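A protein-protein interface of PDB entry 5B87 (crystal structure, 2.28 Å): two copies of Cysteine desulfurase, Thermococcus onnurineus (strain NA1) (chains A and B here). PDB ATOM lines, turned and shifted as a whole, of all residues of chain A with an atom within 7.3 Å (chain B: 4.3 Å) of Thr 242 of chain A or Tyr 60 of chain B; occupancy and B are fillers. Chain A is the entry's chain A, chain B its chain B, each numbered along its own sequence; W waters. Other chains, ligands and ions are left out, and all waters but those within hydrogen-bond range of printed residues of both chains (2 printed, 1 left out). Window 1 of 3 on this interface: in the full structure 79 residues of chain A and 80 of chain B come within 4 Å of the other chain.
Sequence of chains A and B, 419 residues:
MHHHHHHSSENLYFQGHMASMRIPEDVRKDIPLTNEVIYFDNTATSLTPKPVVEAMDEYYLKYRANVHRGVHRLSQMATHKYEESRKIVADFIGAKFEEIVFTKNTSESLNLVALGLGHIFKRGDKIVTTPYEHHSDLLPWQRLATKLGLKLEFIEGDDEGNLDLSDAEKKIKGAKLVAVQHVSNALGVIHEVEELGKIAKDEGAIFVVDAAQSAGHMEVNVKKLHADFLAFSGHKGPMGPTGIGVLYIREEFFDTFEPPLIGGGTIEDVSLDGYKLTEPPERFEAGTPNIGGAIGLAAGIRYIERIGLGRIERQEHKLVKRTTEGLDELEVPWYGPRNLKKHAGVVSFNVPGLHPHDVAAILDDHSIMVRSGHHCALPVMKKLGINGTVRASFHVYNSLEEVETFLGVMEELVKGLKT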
ATOM      1  N   ILE A  31      -1.514   2.436 -31.190  1.00  0.00           N
ATOM      2  CA  ILE A  31      -2.606   3.436 -31.265  1.00  0.00           C
ATOM      3  C   ILE A  31      -2.169   4.580 -32.191  1.00  0.00           C
ATOM      4  O   ILE A  31      -1.539   5.481 -31.724  1.00  0.00           O
ATOM      5  CB  ILE A  31      -3.005   3.973 -29.847  1.00  0.00           C
ATOM      6  CG1 ILE A  31      -3.237   2.793 -28.845  1.00  0.00           C
ATOM      7  CG2 ILE A  31      -4.265   4.854 -29.903  1.00  0.00           C
ATOM      8  CD1 ILE A  31      -3.496   3.237 -27.438  1.00  0.00           C
ATOM      9  N   PRO A  32      -2.511   4.550 -33.497  1.00  0.00           N
ATOM     10  CA  PRO A  32      -2.175   5.629 -34.444  1.00  0.00           C
ATOM     11  C   PRO A  32      -2.480   7.091 -34.015  1.00  0.00           C
ATOM     12  O   PRO A  32      -1.755   8.002 -34.402  1.00  0.00           O
ATOM     13  CB  PRO A  32      -3.005   5.270 -35.693  1.00  0.00           C
ATOM     14  CG  PRO A  32      -3.193   3.802 -35.600  1.00  0.00           C
ATOM     15  CD  PRO A  32      -3.264   3.468 -34.148  1.00  0.00           C
ATOM     16  N   LEU A  33      -3.557   7.311 -33.282  1.00  0.00           N
ATOM     17  CA  LEU A  33      -3.992   8.639 -32.865  1.00  0.00           C
ATOM     18  C   LEU A  33      -2.975   9.296 -31.971  1.00  0.00           C
ATOM     19  O   LEU A  33      -2.823  10.480 -31.919  1.00  0.00           O
ATOM     20  CB  LEU A  33      -5.330   8.550 -32.157  1.00  0.00           C
ATOM     21  CG  LEU A  33      -6.572   9.223 -32.672  1.00  0.00           C
ATOM     22  CD1 LEU A  33      -6.393  10.193 -33.796  1.00  0.00           C
ATOM     23  CD2 LEU A  33      -7.700   8.268 -32.893  1.00  0.00           C
ATOM     24  N   THR A  45     -13.574   8.412 -22.555  1.00  0.00           N
ATOM     25  CA  THR A  45     -13.411   7.175 -23.270  1.00  0.00           C
ATOM     26  C   THR A  45     -11.957   6.960 -23.596  1.00  0.00           C
ATOM     27  O   THR A  45     -11.267   7.875 -23.779  1.00  0.00           O
ATOM     28  CB  THR A  45     -14.302   7.143 -24.529  1.00  0.00           C
ATOM     29  OG1 THR A  45     -14.640   5.812 -24.835  1.00  0.00           O
ATOM     30  CG2 THR A  45     -13.667   7.799 -25.720  1.00  0.00           C
ATOM     31  N   SER A  46     -11.513   5.733 -23.664  1.00  0.00           N
ATOM     32  CA  SER A  46     -10.148   5.488 -24.005  1.00  0.00           C
ATOM     33  C   SER A  46      -9.908   5.428 -25.500  1.00  0.00           C
ATOM     34  O   SER A  46     -10.818   5.419 -26.277  1.00  0.00           O
ATOM     35  CB  SER A  46      -9.687   4.197 -23.393  1.00  0.00           C
ATOM     36  OG  SER A  46     -10.432   3.115 -23.809  1.00  0.00           O
ATOM     37  N   LEU A  47      -8.652   5.386 -25.885  1.00  0.00           N
ATOM     38  CA  LEU A  47      -8.303   5.214 -27.273  1.00  0.00           C
ATOM     39  C   LEU A  47      -8.250   3.716 -27.395  1.00  0.00           C
ATOM     40  O   LEU A  47      -8.054   3.057 -26.436  1.00  0.00           O
ATOM     41  CB  LEU A  47      -6.991   5.867 -27.639  1.00  0.00           C
ATOM     42  CG  LEU A  47      -6.925   7.383 -27.579  1.00  0.00           C
ATOM     43  CD1 LEU A  47      -5.544   7.831 -27.885  1.00  0.00           C
ATOM     44  CD2 LEU A  47      -7.920   8.073 -28.470  1.00  0.00           C
ATOM     45  N   THR A  48      -8.472   3.188 -28.574  1.00  0.00           N
ATOM     46  CA  THR A  48      -8.515   1.756 -28.761  1.00  0.00           C
ATOM     47  C   THR A  48      -7.344   1.151 -29.550  1.00  0.00           C
ATOM     48  O   THR A  48      -7.104   1.509 -30.632  1.00  0.00           O
ATOM     49  CB  THR A  48      -9.906   1.273 -29.237  1.00  0.00           C
ATOM     50  OG1 THR A  48      -9.917   1.173 -30.626  1.00  0.00           O
ATOM     51  CG2 THR A  48     -10.992   2.224 -28.918  1.00  0.00           C
ATOM     52  N   PRO A  49      -6.618   0.239 -28.946  1.00  0.00           N
ATOM     53  CA  PRO A  49      -5.495  -0.381 -29.600  1.00  0.00           C
ATOM     54  C   PRO A  49      -5.894  -1.241 -30.822  1.00  0.00           C
ATOM     55  O   PRO A  49      -6.966  -1.784 -30.869  1.00  0.00           O
ATOM     56  CB  PRO A  49      -4.831  -1.221 -28.499  1.00  0.00           C
ATOM     57  CG  PRO A  49      -5.719  -1.219 -27.355  1.00  0.00           C
ATOM     58  CD  PRO A  49      -6.792  -0.192 -27.560  1.00  0.00           C
ATOM     59  N   VAL A  52      -7.446  -4.773 -30.470  1.00  0.00           N
ATOM     60  CA  VAL A  52      -8.887  -4.757 -30.130  1.00  0.00           C
ATOM     61  C   VAL A  52      -9.723  -4.676 -31.377  1.00  0.00           C
ATOM     62  O   VAL A  52     -10.598  -5.513 -31.565  1.00  0.00           O
ATOM     63  CB  VAL A  52      -9.282  -3.616 -29.163  1.00  0.00           C
ATOM     64  CG1 VAL A  52     -10.753  -3.622 -28.898  1.00  0.00           C
ATOM     65  CG2 VAL A  52      -8.564  -3.757 -27.851  1.00  0.00           C
ATOM     66  N   VAL A  53      -9.408  -3.711 -32.259  1.00  0.00           N
ATOM     67  CA  VAL A  53     -10.138  -3.633 -33.518  1.00  0.00           C
ATOM     68  C   VAL A  53      -9.995  -4.869 -34.440  1.00  0.00           C
ATOM     69  O   VAL A  53     -10.995  -5.382 -34.960  1.00  0.00           O
ATOM     70  CB  VAL A  53     -10.058  -2.255 -34.280  1.00  0.00           C
ATOM     71  CG1 VAL A  53      -9.272  -1.204 -33.573  1.00  0.00           C
ATOM     72  CG2 VAL A  53      -9.697  -2.382 -35.739  1.00  0.00           C
ATOM     73  N   MET A  56     -12.282  -7.643 -33.311  1.00  0.00           N
ATOM     74  CA  MET A  56     -13.693  -7.410 -33.670  1.00  0.00           C
ATOM     75  C   MET A  56     -13.846  -7.622 -35.155  1.00  0.00           C
ATOM     76  O   MET A  56     -14.848  -8.162 -35.579  1.00  0.00           O
ATOM     77  CB  MET A  56     -14.148  -6.002 -33.322  1.00  0.00           C
ATOM     78  CG  MET A  56     -14.017  -5.662 -31.839  1.00  0.00           C
ATOM     79  SD  MET A  56     -14.889  -4.111 -31.519  1.00  0.00           S
ATOM     80  CE  MET A  56     -13.776  -2.920 -32.173  1.00  0.00           C
ATOM     81  N   ASP A  57     -12.860  -7.205 -35.946  1.00  0.00           N
ATOM     82  CA  ASP A  57     -12.916  -7.434 -37.409  1.00  0.00           C
ATOM     83  C   ASP A  57     -12.909  -8.902 -37.796  1.00  0.00           C
ATOM     84  O   ASP A  57     -13.532  -9.227 -38.806  1.00  0.00           O
ATOM     85  CB  ASP A  57     -11.813  -6.689 -38.181  1.00  0.00           C
ATOM     86  CG  ASP A  57     -11.961  -5.175 -38.057  1.00  0.00           C
ATOM     87  OD1 ASP A  57     -12.994  -4.750 -37.494  1.00  0.00           O
ATOM     88  OD2 ASP A  57     -11.063  -4.422 -38.509  1.00  0.00           O
ATOM     89  N   LYS A 104     -25.300  -2.323 -22.553  1.00  0.00           N
ATOM     90  CA  LYS A 104     -24.662  -1.358 -23.454  1.00  0.00           C
ATOM     91  C   LYS A 104     -23.575  -0.415 -22.809  1.00  0.00           C
ATOM     92  O   LYS A 104     -22.569   0.011 -23.447  1.00  0.00           O
ATOM     93  CB  LYS A 104     -25.735  -0.576 -24.224  1.00  0.00           C
ATOM     94  CG  LYS A 104     -26.257   0.710 -23.630  1.00  0.00           C
ATOM     95  CD  LYS A 104     -26.971   1.597 -24.669  1.00  0.00           C
ATOM     96  CE  LYS A 104     -27.708   0.865 -25.809  1.00  0.00           C
ATOM     97  NZ  LYS A 104     -26.900   0.509 -27.067  1.00  0.00           N
ATOM     98  N   ASN A 105     -23.772  -0.132 -21.542  1.00  0.00           N
ATOM     99  CA  ASN A 105     -22.845   0.666 -20.791  1.00  0.00           C
ATOM    100  C   ASN A 105     -23.200   0.593 -19.285  1.00  0.00           C
ATOM    101  O   ASN A 105     -24.191  -0.094 -18.883  1.00  0.00           O
ATOM    102  CB  ASN A 105     -22.913   2.099 -21.297  1.00  0.00           C
ATOM    103  CG  ASN A 105     -24.304   2.633 -21.284  1.00  0.00           C
ATOM    104  OD1 ASN A 105     -25.085   2.279 -20.423  1.00  0.00           O
ATOM    105  ND2 ASN A 105     -24.625   3.505 -22.210  1.00  0.00           N
ATOM    106  N   GLY A 234     -17.006  -0.994 -21.118  1.00  0.00           N
ATOM    107  CA  GLY A 234     -15.877  -1.467 -21.943  1.00  0.00           C
ATOM    108  C   GLY A 234     -15.044  -0.393 -22.597  1.00  0.00           C
ATOM    109  O   GLY A 234     -13.847  -0.566 -22.822  1.00  0.00           O
ATOM    110  N   HIS A 235     -15.688   0.682 -22.996  1.00  0.00           N
ATOM    111  CA  HIS A 235     -15.052   1.761 -23.731  1.00  0.00           C
ATOM    112  C   HIS A 235     -14.122   2.701 -22.996  1.00  0.00           C
ATOM    113  O   HIS A 235     -13.492   3.506 -23.601  1.00  0.00           O
ATOM    114  CB  HIS A 235     -16.099   2.562 -24.507  1.00  0.00           C
ATOM    115  CG  HIS A 235     -16.921   3.457 -23.648  1.00  0.00           C
ATOM    116  ND1 HIS A 235     -16.599   4.765 -23.427  1.00  0.00           N
ATOM    117  CD2 HIS A 235     -18.012   3.207 -22.902  1.00  0.00           C
ATOM    118  CE1 HIS A 235     -17.481   5.294 -22.619  1.00  0.00           C
ATOM    119  NE2 HIS A 235     -18.349   4.369 -22.287  1.00  0.00           N
ATOM    120  N   LYS A 236     -14.052   2.545 -21.750  1.00  0.00           N
ATOM    121  CA  LYS A 236     -13.187   3.360 -20.940  1.00  0.00           C
ATOM    122  C   LYS A 236     -11.840   2.690 -20.674  1.00  0.00           C
ATOM    123  O   LYS A 236     -11.138   2.393 -21.593  1.00  0.00           O
ATOM    124  CB  LYS A 236     -13.919   3.818 -19.682  1.00  0.00           C
ATOM    125  CG  LYS A 236     -15.077   4.719 -19.934  1.00  0.00           C
ATOM    126  CD  LYS A 236     -16.082   5.056 -18.851  1.00  0.00           C
ATOM    127  CE  LYS A 236     -17.183   6.146 -19.182  1.00  0.00           C
ATOM    128  NZ  LYS A 236     -17.506   6.897 -17.955  1.00  0.00           N
ATOM    129  N   GLY A 240     -11.778  -1.299 -24.571  1.00  0.00           N
ATOM    130  CA  GLY A 240     -12.695  -2.023 -25.397  1.00  0.00           C
ATOM    131  C   GLY A 240     -13.482  -1.079 -26.276  1.00  0.00           C
ATOM    132  O   GLY A 240     -13.262   0.080 -26.244  1.00  0.00           O
ATOM    133  N   PRO A 241     -14.426  -1.655 -27.097  1.00  0.00           N
ATOM    134  CA  PRO A 241     -15.180  -0.720 -27.933  1.00  0.00           C
ATOM    135  C   PRO A 241     -16.361  -0.102 -27.220  1.00  0.00           C
ATOM    136  O   PRO A 241     -16.588  -0.432 -26.100  1.00  0.00           O
ATOM    137  CB  PRO A 241     -15.700  -1.618 -29.024  1.00  0.00           C
ATOM    138  CG  PRO A 241     -16.072  -2.812 -28.307  1.00  0.00           C
ATOM    139  CD  PRO A 241     -14.912  -3.068 -27.442  1.00  0.00           C
ATOM    140  N   THR A 242     -17.091   0.776 -27.883  1.00  0.00           N
ATOM    141  CA  THR A 242     -18.353   1.312 -27.362  1.00  0.00           C
ATOM    142  C   THR A 242     -19.487   0.264 -27.427  1.00  0.00           C
ATOM    143  O   THR A 242     -19.383  -0.722 -28.132  1.00  0.00           O
ATOM    144  CB  THR A 242     -18.779   2.565 -28.162  1.00  0.00           C
ATOM    145  OG1 THR A 242     -18.935   2.251 -29.555  1.00  0.00           O
ATOM    146  CG2 THR A 242     -17.732   3.610 -28.075  1.00  0.00           C
ATOM    147  N   GLY A 243     -20.584   0.511 -26.719  1.00  0.00           N
ATOM    148  CA  GLY A 243     -21.754  -0.289 -26.781  1.00  0.00           C
ATOM    149  C   GLY A 243     -21.677  -1.551 -25.925  1.00  0.00           C
ATOM    150  O   GLY A 243     -22.520  -2.407 -26.064  1.00  0.00           O
ATOM    151  N   ILE A 244     -20.664  -1.706 -25.090  1.00  0.00           N
ATOM    152  CA  ILE A 244     -20.564  -2.944 -24.291  1.00  0.00           C
ATOM    153  C   ILE A 244     -20.265  -2.587 -22.845  1.00  0.00           C
ATOM    154  O   ILE A 244     -19.254  -1.999 -22.558  1.00  0.00           O
ATOM    155  CB  ILE A 244     -19.508  -3.920 -24.884  1.00  0.00           C
ATOM    156  CG1 ILE A 244     -19.645  -5.289 -24.244  1.00  0.00           C
ATOM    157  CG2 ILE A 244     -18.086  -3.407 -24.771  1.00  0.00           C
ATOM    158  CD1 ILE A 244     -20.858  -6.047 -24.709  1.00  0.00           C
ATOM    159  N   GLY A 245     -21.220  -2.830 -21.979  1.00  0.00           N
ATOM    160  CA  GLY A 245     -21.055  -2.600 -20.559  1.00  0.00           C
ATOM    161  C   GLY A 245     -21.147  -3.957 -19.909  1.00  0.00           C
ATOM    162  O   GLY A 245     -21.486  -4.977 -20.572  1.00  0.00           O
ATOM    163  N   ASN A 290     -24.529  -8.001 -28.066  1.00  0.00           N
ATOM    164  CA  ASN A 290     -23.492  -7.279 -28.771  1.00  0.00           C
ATOM    165  C   ASN A 290     -22.306  -8.214 -28.839  1.00  0.00           C
ATOM    166  O   ASN A 290     -21.395  -8.139 -28.068  1.00  0.00           O
ATOM    167  CB  ASN A 290     -23.141  -5.977 -28.080  1.00  0.00           C
ATOM    168  CG  ASN A 290     -22.206  -5.136 -28.892  1.00  0.00           C
ATOM    169  OD1 ASN A 290     -21.705  -5.558 -29.890  1.00  0.00           O
ATOM    170  ND2 ASN A 290     -21.971  -3.949 -28.449  1.00  0.00           N
ATOM    171  N   GLY A 292     -19.998  -8.666 -31.191  1.00  0.00           N
ATOM    172  CA  GLY A 292     -18.743  -8.043 -31.610  1.00  0.00           C
ATOM    173  C   GLY A 292     -18.123  -7.202 -30.501  1.00  0.00           C
ATOM    174  O   GLY A 292     -16.899  -7.206 -30.325  1.00  0.00           O
ATOM    175  N   GLY A 293     -18.958  -6.503 -29.740  1.00  0.00           N
ATOM    176  CA  GLY A 293     -18.469  -5.735 -28.549  1.00  0.00           C
ATOM    177  C   GLY A 293     -17.899  -6.573 -27.401  1.00  0.00           C
ATOM    178  O   GLY A 293     -16.857  -6.189 -26.837  1.00  0.00           O
ATOM    179  N   ALA A 294     -18.568  -7.690 -27.043  1.00  0.00           N
ATOM    180  CA  ALA A 294     -18.110  -8.561 -25.974  1.00  0.00           C
ATOM    181  C   ALA A 294     -16.755  -9.140 -26.351  1.00  0.00           C
ATOM    182  O   ALA A 294     -15.835  -9.130 -25.536  1.00  0.00           O
ATOM    183  CB  ALA A 294     -19.096  -9.657 -25.737  1.00  0.00           C
ATOM    184  N   MET B  56     -16.622   1.609 -39.200  1.00  0.00           N
ATOM    185  CA  MET B  56     -16.398   1.445 -37.797  1.00  0.00           C
ATOM    186  C   MET B  56     -14.934   1.525 -37.451  1.00  0.00           C
ATOM    187  O   MET B  56     -14.569   2.129 -36.433  1.00  0.00           O
ATOM    188  CB  MET B  56     -16.922   0.091 -37.343  1.00  0.00           C
ATOM    189  CG  MET B  56     -18.400   0.012 -37.463  1.00  0.00           C
ATOM    190  SD  MET B  56     -19.085  -1.483 -36.706  1.00  0.00           S
ATOM    191  CE  MET B  56     -18.075  -1.771 -35.206  1.00  0.00           C
ATOM    192  N   ASP B  57     -14.103   0.896 -38.293  1.00  0.00           N
ATOM    193  CA  ASP B  57     -12.641   0.940 -38.132  1.00  0.00           C
ATOM    194  C   ASP B  57     -12.180   2.399 -38.201  1.00  0.00           C
ATOM    195  O   ASP B  57     -11.258   2.774 -37.463  1.00  0.00           O
ATOM    196  CB  ASP B  57     -11.880   0.153 -39.210  1.00  0.00           C
ATOM    197  CG  ASP B  57     -11.954  -1.391 -39.035  1.00  0.00           C
ATOM    198  OD1 ASP B  57     -12.457  -1.919 -38.017  1.00  0.00           O
ATOM    199  OD2 ASP B  57     -11.496  -2.094 -39.967  1.00  0.00           O
ATOM    200  N   GLU B  58     -12.778   3.259 -39.023  1.00  0.00           N
ATOM    201  CA  GLU B  58     -12.253   4.654 -38.995  1.00  0.00           C
ATOM    202  C   GLU B  58     -12.606   5.438 -37.710  1.00  0.00           C
ATOM    203  O   GLU B  58     -11.785   6.228 -37.245  1.00  0.00           O
ATOM    204  CB  GLU B  58     -12.325   5.448 -40.311  1.00  0.00           C
ATOM    205  CG  GLU B  58     -13.650   5.699 -40.939  1.00  0.00           C
ATOM    206  CD  GLU B  58     -13.775   7.078 -41.641  1.00  0.00           C
ATOM    207  OE1 GLU B  58     -12.753   7.736 -42.025  1.00  0.00           O
ATOM    208  OE2 GLU B  58     -14.938   7.482 -41.800  1.00  0.00           O
ATOM    209  N   TYR B  59     -13.777   5.180 -37.104  1.00  0.00           N
ATOM    210  CA  TYR B  59     -14.077   5.792 -35.796  1.00  0.00           C
ATOM    211  C   TYR B  59     -13.075   5.275 -34.765  1.00  0.00           C
ATOM    212  O   TYR B  59     -12.462   6.022 -34.023  1.00  0.00           O
ATOM    213  CB  TYR B  59     -15.493   5.462 -35.345  1.00  0.00           C
ATOM    214  CG  TYR B  59     -15.706   5.694 -33.895  1.00  0.00           C
ATOM    215  CD1 TYR B  59     -15.763   7.000 -33.403  1.00  0.00           C
ATOM    216  CD2 TYR B  59     -15.853   4.647 -33.006  1.00  0.00           C
ATOM    217  CE1 TYR B  59     -15.984   7.248 -32.088  1.00  0.00           C
ATOM    218  CE2 TYR B  59     -16.077   4.887 -31.661  1.00  0.00           C
ATOM    219  CZ  TYR B  59     -16.124   6.195 -31.217  1.00  0.00           C
ATOM    220  OH  TYR B  59     -16.330   6.502 -29.925  1.00  0.00           O
ATOM    221  N   TYR B  60     -12.879   3.989 -34.723  1.00  0.00           N
ATOM    222  CA  TYR B  60     -11.932   3.468 -33.756  1.00  0.00           C
ATOM    223  C   TYR B  60     -10.497   3.932 -33.908  1.00  0.00           C
ATOM    224  O   TYR B  60      -9.824   4.269 -32.931  1.00  0.00           O
ATOM    225  CB  TYR B  60     -12.065   1.968 -33.632  1.00  0.00           C
ATOM    226  CG  TYR B  60     -13.337   1.577 -32.907  1.00  0.00           C
ATOM    227  CD1 TYR B  60     -13.522   1.960 -31.599  1.00  0.00           C
ATOM    228  CD2 TYR B  60     -14.328   0.770 -33.510  1.00  0.00           C
ATOM    229  CE1 TYR B  60     -14.671   1.632 -30.906  1.00  0.00           C
ATOM    230  CE2 TYR B  60     -15.500   0.450 -32.804  1.00  0.00           C
ATOM    231  CZ  TYR B  60     -15.642   0.887 -31.486  1.00  0.00           C
ATOM    232  OH  TYR B  60     -16.750   0.644 -30.710  1.00  0.00           O
ATOM    233  N   LEU B  61     -10.019   4.012 -35.110  1.00  0.00           N
ATOM    234  CA  LEU B  61      -8.594   4.318 -35.279  1.00  0.00           C
ATOM    235  C   LEU B  61      -8.267   5.785 -35.597  1.00  0.00           C
ATOM    236  O   LEU B  61      -7.155   6.175 -35.327  1.00  0.00           O
ATOM    237  CB  LEU B  61      -7.991   3.401 -36.372  1.00  0.00           C
ATOM    238  CG  LEU B  61      -8.008   1.881 -35.983  1.00  0.00           C
ATOM    239  CD1 LEU B  61      -7.561   0.915 -37.107  1.00  0.00           C
ATOM    240  CD2 LEU B  61      -7.155   1.698 -34.739  1.00  0.00           C
ATOM    241  N   LYS B  62      -9.198   6.554 -36.174  1.00  0.00           N
ATOM    242  CA  LYS B  62      -8.927   7.928 -36.668  1.00  0.00           C
ATOM    243  C   LYS B  62      -9.682   9.022 -35.951  1.00  0.00           C
ATOM    244  O   LYS B  62      -9.173  10.095 -35.929  1.00  0.00           O
ATOM    245  CB  LYS B  62      -9.194   8.056 -38.154  1.00  0.00           C
ATOM    246  CG  LYS B  62      -8.100   7.381 -39.016  1.00  0.00           C
ATOM    247  CD  LYS B  62      -8.354   7.555 -40.533  1.00  0.00           C
ATOM    248  CE  LYS B  62      -7.151   7.215 -41.403  1.00  0.00           C
ATOM    249  NZ  LYS B  62      -6.774   5.796 -41.205  1.00  0.00           N
ATOM    250  N   ARG B  64     -11.543   8.498 -32.648  1.00  0.00           N
ATOM    251  CA  ARG B  64     -12.034   7.946 -31.431  1.00  0.00           C
ATOM    252  C   ARG B  64     -12.227   8.950 -30.279  1.00  0.00           C
ATOM    253  O   ARG B  64     -11.304   9.548 -29.810  1.00  0.00           O
ATOM    254  CB  ARG B  64     -11.194   6.732 -31.052  1.00  0.00           C
ATOM    255  CG  ARG B  64     -11.617   5.990 -29.816  1.00  0.00           C
ATOM    256  CD  ARG B  64     -12.754   5.020 -30.006  1.00  0.00           C
ATOM    257  NE  ARG B  64     -12.881   4.244 -28.802  1.00  0.00           N
ATOM    258  CZ  ARG B  64     -13.654   4.538 -27.786  1.00  0.00           C
ATOM    259  NH1 ARG B  64     -13.628   3.812 -26.734  1.00  0.00           N
ATOM    260  NH2 ARG B  64     -14.474   5.534 -27.833  1.00  0.00           N
ATOM    261  N   PRO B 289     -23.413   6.268 -25.764  1.00  0.00           N
ATOM    262  CA  PRO B 289     -24.083   5.374 -26.699  1.00  0.00           C
ATOM    263  C   PRO B 289     -23.099   4.530 -27.467  1.00  0.00           C
ATOM    264  O   PRO B 289     -21.930   4.787 -27.402  1.00  0.00           O
ATOM    265  CB  PRO B 289     -24.844   6.322 -27.597  1.00  0.00           C
ATOM    266  CG  PRO B 289     -24.158   7.608 -27.473  1.00  0.00           C
ATOM    267  CD  PRO B 289     -23.474   7.670 -26.168  1.00  0.00           C
ATOM    268  N   ASN B 290     -23.576   3.511 -28.152  1.00  0.00           N
ATOM    269  CA  ASN B 290     -22.729   2.671 -28.954  1.00  0.00           C
ATOM    270  C   ASN B 290     -22.421   3.461 -30.200  1.00  0.00           C
ATOM    271  O   ASN B 290     -23.013   3.296 -31.211  1.00  0.00           O
ATOM    272  CB  ASN B 290     -23.390   1.353 -29.281  1.00  0.00           C
ATOM    273  CG  ASN B 290     -22.483   0.419 -30.026  1.00  0.00           C
ATOM    274  OD1 ASN B 290     -21.365   0.707 -30.279  1.00  0.00           O
ATOM    275  ND2 ASN B 290     -22.983  -0.703 -30.358  1.00  0.00           N
ATOM    276  N   ILE B 291     -21.462   4.343 -30.072  1.00  0.00           N
ATOM    277  CA  ILE B 291     -21.046   5.214 -31.123  1.00  0.00           C
ATOM    278  C   ILE B 291     -20.611   4.456 -32.338  1.00  0.00           C
ATOM    279  O   ILE B 291     -21.060   4.730 -33.392  1.00  0.00           O
ATOM    280  CB  ILE B 291     -19.967   6.203 -30.650  1.00  0.00           C
ATOM    281  CG1 ILE B 291     -20.488   7.064 -29.528  1.00  0.00           C
ATOM    282  CG2 ILE B 291     -19.506   7.102 -31.767  1.00  0.00           C
ATOM    283  CD1 ILE B 291     -19.427   7.592 -28.626  1.00  0.00           C
ATOM    284  N   GLY B 292     -19.743   3.501 -32.152  1.00  0.00           N
ATOM    285  CA  GLY B 292     -19.258   2.698 -33.222  1.00  0.00           C
ATOM    286  C   GLY B 292     -20.352   1.970 -33.931  1.00  0.00           C
ATOM    287  O   GLY B 292     -20.353   1.911 -35.106  1.00  0.00           O
HETATM  288  O   HOH W   1     -10.639  -4.262 -41.839  1.00  0.00           O
HETATM  289  O   HOH W   2     -21.527   2.349 -24.949  1.00  0.00           O
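NH1 of Arg 64 of chain B sits at hydrogen-bond distance from OG1 of Thr 45 of chain A, at 2.9 Å. The side-chain hydroxyl of Thr 242 of chain A sits at hydrogen-bond distance from the backbone NH of Gly 292 of chain B (3.0 Å). The backbone carbonyl oxygen (O) of Ser 46 of chain A is in hydrogen-bond range of the guanidinium group (NH1) of Arg 64 of chain B. OD2 of Asp 57 of chain B sits close to OD2 of Asp 57 of chain A (2.8 Å). The backbone carbonyl oxygen (O) of His 235 of chain A lies within hydrogen-bond range of the guanidinium group (NH1) of Arg 64 of chain B (3.2 Å). The backbone NH of Thr 242 of chain A is in hydrogen-bond range of the side-chain hydroxyl of Tyr 60 of chain B, 2.9 Å away. The backbone NH (N) of Ile 291 of chain B lies within hydrogen-bond range of the side-chain hydroxyl (OG1) of Thr 242 of chain A (3.3 Å). The side-chain amide oxygen (OD1) of Asn 290 of chain B is in hydrogen-bond range of the side-chain hydroxyl (OG1) of Thr 242 of chain A.
A ring nitrogen (ND1) of His 235 of chain A is in hydrogen-bond range of the side-chain hydroxyl of Thr 45 of chain A (2.6 Å). The side-chain hydroxyl (OH) of Tyr 59 of chain B sits at hydrogen-bond distance from the guanidinium group (NH2) of Arg 64 of chain B, 3.0 Å away. The backbone carbonyl oxygen (O) of His 235 of chain A lies within hydrogen-bond range of the backbone NH (N) of Ser 46 of chain A (3.0 Å).
Among the printed residues, pairs that only touch across the chains: Leu 33 of chain A with Leu 61 of chain B, Leu 33 of chain A with Lys 62 of chain B, Leu 33 of chain A with Arg 64 of chain B, Leu 47 of chain A with Arg 64 of chain B, Thr 48 of chain A with Tyr 60 of chain B, Thr 48 of chain A with Arg 64 of chain B, Val 53 of chain A with Asp 57 of chain B, Val 53 of chain A with Leu 61 of chain B, Met 56 of chain A with Tyr 60 of chain B, Gly 240 of chain A with Arg 64 of chain B, Pro 241 of chain A with Tyr 60 of chain B, Thr 242 of chain A with Tyr 59 of chain B, Thr 242 of chain A with Arg 64 of chain B, Thr 242 of chain A with Pro 289 of chain B, Gly 243 of chain A with Asn 290 of chain B and Asn 290 of chain A with Asn 290 of chain B.
Of the printed residues of chain B, Leu 47 of chain A touches Arg 64. Of the printed residues of chain B, Asp 57 of chain A touches Asp 57. Of the printed residues of chain B, Thr 242 of chain A touches Tyr 59 (3.7 Å), Tyr 60 (2.9 Å), Arg 64 (3.8 Å), Pro 289 (3.9 Å), Asn 290 (3.0 Å), Ile 291 (3.3 Å) and Gly 292 (3.0 Å). Gly 293 of chain A touches none of the printed residues of chain B. Of chain A, only Thr 48 (3.7 Å), Met 56 (3.8 Å), Pro 241 (3.0 Å) and Thr 242 (2.9 Å) come within 4 Å of Tyr 60 of chain B.
Printed residues of chain A that touch a printed residue of chain B: Leu 33, Thr 45, Ser 46, Leu 47, Thr 48, Val 53, Met 56, Asp 57, His 235, Gly 240, Pro 241, Thr 242, Gly 243 and Asn 290. Hydrophobic or aromatic side chains of chain A within 4 Å of the printed part of chain B: Leu 33, Leu 47, Val 53, Met 56, His 235 and Pro 241. Hydrophobic or aromatic side chains of chain B that line the printed part of chain A: Tyr 59, Tyr 60 and Leu 61. Among the printed residues, 24 pairs touch across the chains.
Asp 57 of chain B touches its own counterpart, Asp 57 of chain A. Asn 290 of chain A touches its own counterpart, Asn 290 of chain B. 4 positions are printed for both chains.
Water W2 lies within hydrogen-bond range of N of Gly 243 of chain A (2.7 Å), O of Lys 104 of chain A (3.0 Å) and O of Pro 289 of chain B (3.5 Å). Water W1 bridges the side-chain carboxylate of Asp 57 of chain B (3.0 Å) and the side-chain carboxylate of Asp 57 of chain A (3.4 Å).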
